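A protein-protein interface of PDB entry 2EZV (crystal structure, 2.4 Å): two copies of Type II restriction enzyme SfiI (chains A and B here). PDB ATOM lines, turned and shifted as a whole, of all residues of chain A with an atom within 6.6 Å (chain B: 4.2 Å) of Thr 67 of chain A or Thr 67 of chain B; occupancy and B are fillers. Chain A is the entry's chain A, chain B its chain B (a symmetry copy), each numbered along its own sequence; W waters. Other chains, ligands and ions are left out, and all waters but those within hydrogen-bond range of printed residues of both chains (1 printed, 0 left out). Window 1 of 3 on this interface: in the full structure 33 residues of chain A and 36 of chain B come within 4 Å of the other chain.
The backbone NH of Tyr 68 of chain A lies within hydrogen-bond range of the backbone carbonyl oxygen of Glu 66 of chain B, at 3.0 Å. The backbone carbonyl oxygen of Glu 66 of chain A sits at hydrogen-bond distance from the backbone NH of Tyr 68 of chain B, at 2.9 Å.
The side-chain carboxylate (OE2) of Glu 66 of chain A lies within salt-bridge range of the guanidinium group (NH1) of Arg 84 of chain A, 2.8 Å away. The backbone NH (N) of Trp 85 of chain B sits at hydrogen-bond distance from the backbone carbonyl oxygen (O) of Tyr 68 of chain B. The side-chain hydroxyl of Thr 67 of chain A is in hydrogen-bond range of the backbone carbonyl oxygen of Trp 85 of chain A (2.9 Å). The backbone carbonyl oxygen of Tyr 68 of chain A lies within hydrogen-bond range of the backbone NH of Trp 85 of chain A (2.9 Å). OE2 of Glu 66 of chain B is in salt-bridge range of NH1 of Arg 84 of chain B (2.5 Å). OG1 of Thr 67 of chain B sits at hydrogen-bond distance from O of Trp 85 of chain B (2.8 Å).
Among the printed residues, merely in contact across the chains: Ala 65 of chain A with Tyr 68 of chain B, Glu 66 of chain A with Thr 67 of chain B, Thr 67 of chain A with Glu 66 of chain B, Val 64 of chain A with Pro 69 of chain B, Val 64 of chain A with Tyr 68 of chain B, Thr 67 of chain A with Thr 67 of chain B and Thr 23 of chain A with Tyr 68 of chain B.
Of chain B, only Glu 66 (3.6 Å) and Thr 67 (3.6 Å) come within 4 Å of Thr 67 of chain A. Thr 67 of chain B touches two residues of chain A. Of the printed residues of chain B, Glu 66 of chain A touches Thr 67 and Tyr 68. Of the printed residues of chain B, Thr 23 of chain A touches Tyr 68. Of the printed residues of chain A, Tyr 68 of chain B touches Thr 23, Val 64, Ala 65 and Glu 66. Printed residues of chain A within 4 Å of Glu 66 of chain B: Thr 67 (3.6 Å) and Tyr 68 (3.0 Å). Of the printed residues of chain B, Ala 65 of chain A touches Tyr 68 (3.3 Å). The nearest printed residue of chain B that does not touch Thr 67 of chain A is Tyr 68 of chain B (4.6 Å). The nearest residue of chain A that does not touch Thr 67 of chain B is Pro 87 of chain A (4.2 Å).
Printed residues of chain A that touch a printed residue of chain B: Thr 23, Val 64, Ala 65, Glu 66, Thr 67 and Tyr 68. Hydrophobic or aromatic side chains of chain A that line the printed part of chain B: Ala 65. Among the printed residues, 9 pairs touch across the chains.
Glu 66 of chain A touches Thr 67 of chain B, and with the chains exchanged Thr 67 of chain A touches Glu 66 of chain B. Glu 66 of chain A touches Tyr 68 of chain B, and with the chains exchanged Tyr 68 of chain A touches Glu 66 of chain B. Thr 67 of chain A touches its own counterpart, Thr 67 of chain B. 6 positions are printed for both chains.
Water W1 bridges the backbone carbonyl oxygen of Pro 69 of chain B (2.8 Å) and the backbone carbonyl oxygen of Val 64 of chain A (2.8 Å).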
ATOM      1  N   THR A  23      -6.399 -15.699  19.472  1.00  0.00           N
ATOM      2  CA  THR A  23      -5.057 -15.343  19.928  1.00  0.00           C
ATOM      3  C   THR A  23      -4.466 -16.483  20.744  1.00  0.00           C
ATOM      4  O   THR A  23      -3.297 -16.839  20.592  1.00  0.00           O
ATOM      5  CB  THR A  23      -5.080 -14.080  20.821  1.00  0.00           C
ATOM      6  OG1 THR A  23      -5.605 -12.976  20.077  1.00  0.00           O
ATOM      7  CG2 THR A  23      -3.676 -13.740  21.308  1.00  0.00           C
ATOM      8  N   VAL A  64       3.139 -15.294  26.992  1.00  0.00           N
ATOM      9  CA  VAL A  64       3.948 -14.753  25.918  1.00  0.00           C
ATOM     10  C   VAL A  64       3.113 -14.040  24.840  1.00  0.00           C
ATOM     11  O   VAL A  64       3.648 -13.369  23.960  1.00  0.00           O
ATOM     12  CB  VAL A  64       4.765 -15.923  25.317  1.00  0.00           C
ATOM     13  CG1 VAL A  64       4.287 -16.263  23.920  1.00  0.00           C
ATOM     14  CG2 VAL A  64       6.238 -15.611  25.381  1.00  0.00           C
ATOM     15  N   ALA A  65       1.794 -14.163  24.925  1.00  0.00           N
ATOM     16  CA  ALA A  65       0.918 -13.559  23.930  1.00  0.00           C
ATOM     17  C   ALA A  65      -0.101 -12.602  24.533  1.00  0.00           C
ATOM     18  O   ALA A  65      -1.216 -12.497  24.036  1.00  0.00           O
ATOM     19  CB  ALA A  65       0.193 -14.661  23.154  1.00  0.00           C
ATOM     20  N   GLU A  66       0.282 -11.908  25.599  1.00  0.00           N
ATOM     21  CA  GLU A  66      -0.610 -10.963  26.256  1.00  0.00           C
ATOM     22  C   GLU A  66      -0.701  -9.616  25.542  1.00  0.00           C
ATOM     23  O   GLU A  66      -0.016  -9.375  24.543  1.00  0.00           O
ATOM     24  CB  GLU A  66      -0.166 -10.745  27.704  1.00  0.00           C
ATOM     25  CG  GLU A  66      -0.587 -11.878  28.612  1.00  0.00           C
ATOM     26  CD  GLU A  66      -2.098 -11.990  28.684  1.00  0.00           C
ATOM     27  OE1 GLU A  66      -2.614 -13.080  29.001  1.00  0.00           O
ATOM     28  OE2 GLU A  66      -2.769 -10.970  28.424  1.00  0.00           O
ATOM     29  N   THR A  67      -1.558  -8.748  26.068  1.00  0.00           N
ATOM     30  CA  THR A  67      -1.751  -7.415  25.515  1.00  0.00           C
ATOM     31  C   THR A  67      -1.813  -6.367  26.627  1.00  0.00           C
ATOM     32  O   THR A  67      -2.085  -6.692  27.777  1.00  0.00           O
ATOM     33  CB  THR A  67      -3.076  -7.319  24.729  1.00  0.00           C
ATOM     34  OG1 THR A  67      -4.171  -7.562  25.623  1.00  0.00           O
ATOM     35  CG2 THR A  67      -3.113  -8.336  23.599  1.00  0.00           C
ATOM     36  N   TYR A  68      -1.546  -5.120  26.242  1.00  0.00           N
ATOM     37  CA  TYR A  68      -1.604  -3.920  27.083  1.00  0.00           C
ATOM     38  C   TYR A  68      -2.101  -4.187  28.511  1.00  0.00           C
ATOM     39  O   TYR A  68      -3.289  -4.089  28.778  1.00  0.00           O
ATOM     40  CB  TYR A  68      -2.532  -2.941  26.362  1.00  0.00           C
ATOM     41  CG  TYR A  68      -2.529  -1.483  26.778  1.00  0.00           C
ATOM     42  CD1 TYR A  68      -3.179  -0.539  25.981  1.00  0.00           C
ATOM     43  CD2 TYR A  68      -1.921  -1.043  27.963  1.00  0.00           C
ATOM     44  CE1 TYR A  68      -3.233   0.800  26.338  1.00  0.00           C
ATOM     45  CE2 TYR A  68      -1.971   0.313  28.330  1.00  0.00           C
ATOM     46  CZ  TYR A  68      -2.629   1.221  27.504  1.00  0.00           C
ATOM     47  OH  TYR A  68      -2.681   2.557  27.817  1.00  0.00           O
ATOM     48  N   PRO A  69      -1.191  -4.510  29.449  1.00  0.00           N
ATOM     49  CA  PRO A  69      -1.563  -4.793  30.842  1.00  0.00           C
ATOM     50  C   PRO A  69      -2.157  -3.633  31.633  1.00  0.00           C
ATOM     51  O   PRO A  69      -1.777  -2.467  31.453  1.00  0.00           O
ATOM     52  CB  PRO A  69      -0.250  -5.280  31.470  1.00  0.00           C
ATOM     53  CG  PRO A  69       0.528  -5.823  30.289  1.00  0.00           C
ATOM     54  CD  PRO A  69       0.243  -4.768  29.234  1.00  0.00           C
ATOM     55  N   ILE A  70      -3.102  -3.968  32.508  1.00  0.00           N
ATOM     56  CA  ILE A  70      -3.735  -2.983  33.361  1.00  0.00           C
ATOM     57  C   ILE A  70      -3.183  -3.241  34.743  1.00  0.00           C
ATOM     58  O   ILE A  70      -2.977  -4.391  35.127  1.00  0.00           O
ATOM     59  CB  ILE A  70      -5.275  -3.118  33.362  1.00  0.00           C
ATOM     60  CG1 ILE A  70      -5.832  -2.501  32.078  1.00  0.00           C
ATOM     61  CG2 ILE A  70      -5.860  -2.429  34.582  1.00  0.00           C
ATOM     62  CD1 ILE A  70      -7.300  -2.711  31.867  1.00  0.00           C
ATOM     63  N   VAL A  83      -5.602  -8.915  33.858  1.00  0.00           N
ATOM     64  CA  VAL A  83      -6.519  -7.810  33.605  1.00  0.00           C
ATOM     65  C   VAL A  83      -5.756  -7.011  32.538  1.00  0.00           C
ATOM     66  O   VAL A  83      -4.545  -6.797  32.663  1.00  0.00           O
ATOM     67  CB  VAL A  83      -6.737  -6.950  34.877  1.00  0.00           C
ATOM     68  CG1 VAL A  83      -7.837  -5.936  34.637  1.00  0.00           C
ATOM     69  CG2 VAL A  83      -7.110  -7.836  36.060  1.00  0.00           C
ATOM     70  N   ARG A  84      -6.445  -6.568  31.493  1.00  0.00           N
ATOM     71  CA  ARG A  84      -5.757  -5.870  30.410  1.00  0.00           C
ATOM     72  C   ARG A  84      -6.712  -5.123  29.491  1.00  0.00           C
ATOM     73  O   ARG A  84      -7.923  -5.179  29.670  1.00  0.00           O
ATOM     74  CB  ARG A  84      -5.036  -6.907  29.567  1.00  0.00           C
ATOM     75  CG  ARG A  84      -6.045  -7.838  28.893  1.00  0.00           C
ATOM     76  CD  ARG A  84      -5.404  -9.031  28.229  1.00  0.00           C
ATOM     77  NE  ARG A  84      -6.364  -9.722  27.380  1.00  0.00           N
ATOM     78  CZ  ARG A  84      -6.088 -10.795  26.647  1.00  0.00           C
ATOM     79  NH1 ARG A  84      -4.868 -11.316  26.655  1.00  0.00           N
ATOM     80  NH2 ARG A  84      -7.036 -11.344  25.897  1.00  0.00           N
ATOM     81  N   TRP A  85      -6.154  -4.423  28.505  1.00  0.00           N
ATOM     82  CA  TRP A  85      -6.969  -3.735  27.502  1.00  0.00           C
ATOM     83  C   TRP A  85      -6.866  -4.623  26.266  1.00  0.00           C
ATOM     84  O   TRP A  85      -5.781  -5.137  25.955  1.00  0.00           O
ATOM     85  CB  TRP A  85      -6.411  -2.361  27.126  1.00  0.00           C
ATOM     86  CG  TRP A  85      -6.436  -1.329  28.186  1.00  0.00           C
ATOM     87  CD1 TRP A  85      -5.391  -0.936  28.971  1.00  0.00           C
ATOM     88  CD2 TRP A  85      -7.532  -0.471  28.517  1.00  0.00           C
ATOM     89  NE1 TRP A  85      -5.764   0.124  29.763  1.00  0.00           N
ATOM     90  CE2 TRP A  85      -7.072   0.432  29.505  1.00  0.00           C
ATOM     91  CE3 TRP A  85      -8.857  -0.371  28.073  1.00  0.00           C
ATOM     92  CZ2 TRP A  85      -7.889   1.422  30.052  1.00  0.00           C
ATOM     93  CZ3 TRP A  85      -9.673   0.615  28.617  1.00  0.00           C
ATOM     94  CH2 TRP A  85      -9.184   1.502  29.599  1.00  0.00           C
ATOM     95  N   LEU A  86      -7.980  -4.794  25.566  1.00  0.00           N
ATOM     96  CA  LEU A  86      -8.019  -5.611  24.364  1.00  0.00           C
ATOM     97  C   LEU A  86      -8.344  -4.743  23.160  1.00  0.00           C
ATOM     98  O   LEU A  86      -9.488  -4.307  22.987  1.00  0.00           O
ATOM     99  CB  LEU A  86      -9.084  -6.701  24.494  1.00  0.00           C
ATOM    100  CG  LEU A  86      -9.272  -7.588  23.264  1.00  0.00           C
ATOM    101  CD1 LEU A  86      -7.956  -8.311  22.971  1.00  0.00           C
ATOM    102  CD2 LEU A  86     -10.396  -8.582  23.506  1.00  0.00           C
ATOM    103  N   PRO A  87      -7.340  -4.461  22.315  1.00  0.00           N
ATOM    104  CA  PRO A  87      -7.645  -3.626  21.153  1.00  0.00           C
ATOM    105  C   PRO A  87      -8.725  -4.263  20.280  1.00  0.00           C
ATOM    106  O   PRO A  87      -8.683  -5.455  19.964  1.00  0.00           O
ATOM    107  CB  PRO A  87      -6.286  -3.471  20.456  1.00  0.00           C
ATOM    108  CG  PRO A  87      -5.471  -4.612  20.960  1.00  0.00           C
ATOM    109  CD  PRO A  87      -5.898  -4.745  22.401  1.00  0.00           C
ATOM    110  N   GLN A  95     -10.420  -5.772  29.877  1.00  0.00           N
ATOM    111  CA  GLN A  95     -10.827  -7.162  30.006  1.00  0.00           C
ATOM    112  C   GLN A  95     -10.100  -7.967  31.062  1.00  0.00           C
ATOM    113  O   GLN A  95      -8.953  -7.699  31.378  1.00  0.00           O
ATOM    114  CB  GLN A  95     -10.644  -7.850  28.649  1.00  0.00           C
ATOM    115  CG  GLN A  95     -10.712  -9.369  28.645  1.00  0.00           C
ATOM    116  CD  GLN A  95     -10.298  -9.953  27.295  1.00  0.00           C
ATOM    117  OE1 GLN A  95      -9.159  -9.766  26.848  1.00  0.00           O
ATOM    118  NE2 GLN A  95     -11.220 -10.652  26.638  1.00  0.00           N
ATOM    119  N   GLU B  66       1.950  -2.700  24.411  1.00  0.00           N
ATOM    120  CA  GLU B  66       2.207  -3.553  23.250  1.00  0.00           C
ATOM    121  C   GLU B  66       1.379  -4.853  23.262  1.00  0.00           C
ATOM    122  O   GLU B  66       0.667  -5.132  24.231  1.00  0.00           O
ATOM    123  CB  GLU B  66       3.706  -3.863  23.204  1.00  0.00           C
ATOM    124  CG  GLU B  66       4.270  -4.089  21.815  1.00  0.00           C
ATOM    125  CD  GLU B  66       3.940  -2.975  20.848  1.00  0.00           C
ATOM    126  OE1 GLU B  66       4.426  -1.834  21.011  1.00  0.00           O
ATOM    127  OE2 GLU B  66       3.178  -3.251  19.910  1.00  0.00           O
ATOM    128  N   THR B  67       1.446  -5.624  22.174  1.00  0.00           N
ATOM    129  CA  THR B  67       0.719  -6.896  22.102  1.00  0.00           C
ATOM    130  C   THR B  67       1.559  -8.061  21.578  1.00  0.00           C
ATOM    131  O   THR B  67       2.600  -7.862  20.960  1.00  0.00           O
ATOM    132  CB  THR B  67      -0.555  -6.815  21.199  1.00  0.00           C
ATOM    133  OG1 THR B  67      -0.178  -6.587  19.832  1.00  0.00           O
ATOM    134  CG2 THR B  67      -1.488  -5.715  21.676  1.00  0.00           C
ATOM    135  N   TYR B  68       1.074  -9.274  21.859  1.00  0.00           N
ATOM    136  CA  TYR B  68       1.650 -10.550  21.431  1.00  0.00           C
ATOM    137  C   TYR B  68       2.841 -10.380  20.484  1.00  0.00           C
ATOM    138  O   TYR B  68       2.676 -10.386  19.266  1.00  0.00           O
ATOM    139  CB  TYR B  68       0.534 -11.339  20.740  1.00  0.00           C
ATOM    140  CG  TYR B  68       0.797 -12.797  20.445  1.00  0.00           C
ATOM    141  CD1 TYR B  68      -0.213 -13.593  19.901  1.00  0.00           C
ATOM    142  CD2 TYR B  68       2.036 -13.390  20.720  1.00  0.00           C
ATOM    143  CE1 TYR B  68      -0.003 -14.951  19.637  1.00  0.00           C
ATOM    144  CE2 TYR B  68       2.259 -14.748  20.463  1.00  0.00           C
ATOM    145  CZ  TYR B  68       1.232 -15.523  19.923  1.00  0.00           C
ATOM    146  OH  TYR B  68       1.424 -16.871  19.690  1.00  0.00           O
ATOM    147  N   PRO B  69       4.057 -10.245  21.033  1.00  0.00           N
ATOM    148  CA  PRO B  69       5.261 -10.068  20.214  1.00  0.00           C
ATOM    149  C   PRO B  69       5.622 -11.199  19.245  1.00  0.00           C
ATOM    150  O   PRO B  69       5.406 -12.387  19.518  1.00  0.00           O
ATOM    151  CB  PRO B  69       6.374  -9.855  21.255  1.00  0.00           C
ATOM    152  CG  PRO B  69       5.648  -9.311  22.454  1.00  0.00           C
ATOM    153  CD  PRO B  69       4.395 -10.172  22.468  1.00  0.00           C
ATOM    154  N   ARG B  84       4.541  -7.588  15.647  1.00  0.00           N
ATOM    155  CA  ARG B  84       3.684  -8.244  16.627  1.00  0.00           C
ATOM    156  C   ARG B  84       2.402  -8.795  16.004  1.00  0.00           C
ATOM    157  O   ARG B  84       2.127  -8.567  14.836  1.00  0.00           O
ATOM    158  CB  ARG B  84       3.287  -7.210  17.682  1.00  0.00           C
ATOM    159  CG  ARG B  84       2.430  -6.097  17.056  1.00  0.00           C
ATOM    160  CD  ARG B  84       2.119  -4.918  17.954  1.00  0.00           C
ATOM    161  NE  ARG B  84       1.070  -4.111  17.330  1.00  0.00           N
ATOM    162  CZ  ARG B  84       0.528  -3.010  17.851  1.00  0.00           C
ATOM    163  NH1 ARG B  84       0.938  -2.544  19.020  1.00  0.00           N
ATOM    164  NH2 ARG B  84      -0.465  -2.398  17.215  1.00  0.00           N
ATOM    165  N   TRP B  85       1.624  -9.521  16.804  1.00  0.00           N
ATOM    166  CA  TRP B  85       0.340 -10.061  16.365  1.00  0.00           C
ATOM    167  C   TRP B  85      -0.718  -9.110  16.915  1.00  0.00           C
ATOM    168  O   TRP B  85      -0.697  -8.763  18.098  1.00  0.00           O
ATOM    169  CB  TRP B  85       0.068 -11.451  16.955  1.00  0.00           C
ATOM    170  CG  TRP B  85       0.900 -12.566  16.416  1.00  0.00           C
ATOM    171  CD1 TRP B  85       1.931 -13.190  17.042  1.00  0.00           C
ATOM    172  CD2 TRP B  85       0.701 -13.260  15.177  1.00  0.00           C
ATOM    173  NE1 TRP B  85       2.384 -14.242  16.280  1.00  0.00           N
ATOM    174  CE2 TRP B  85       1.646 -14.309  15.131  1.00  0.00           C
ATOM    175  CE3 TRP B  85      -0.193 -13.102  14.105  1.00  0.00           C
ATOM    176  CZ2 TRP B  85       1.726 -15.202  14.054  1.00  0.00           C
ATOM    177  CZ3 TRP B  85      -0.113 -13.994  13.032  1.00  0.00           C
ATOM    178  CH2 TRP B  85       0.841 -15.030  13.019  1.00  0.00           C
HETATM  179  O   HOH W   1       5.610 -13.738  21.934  1.00  0.00           O
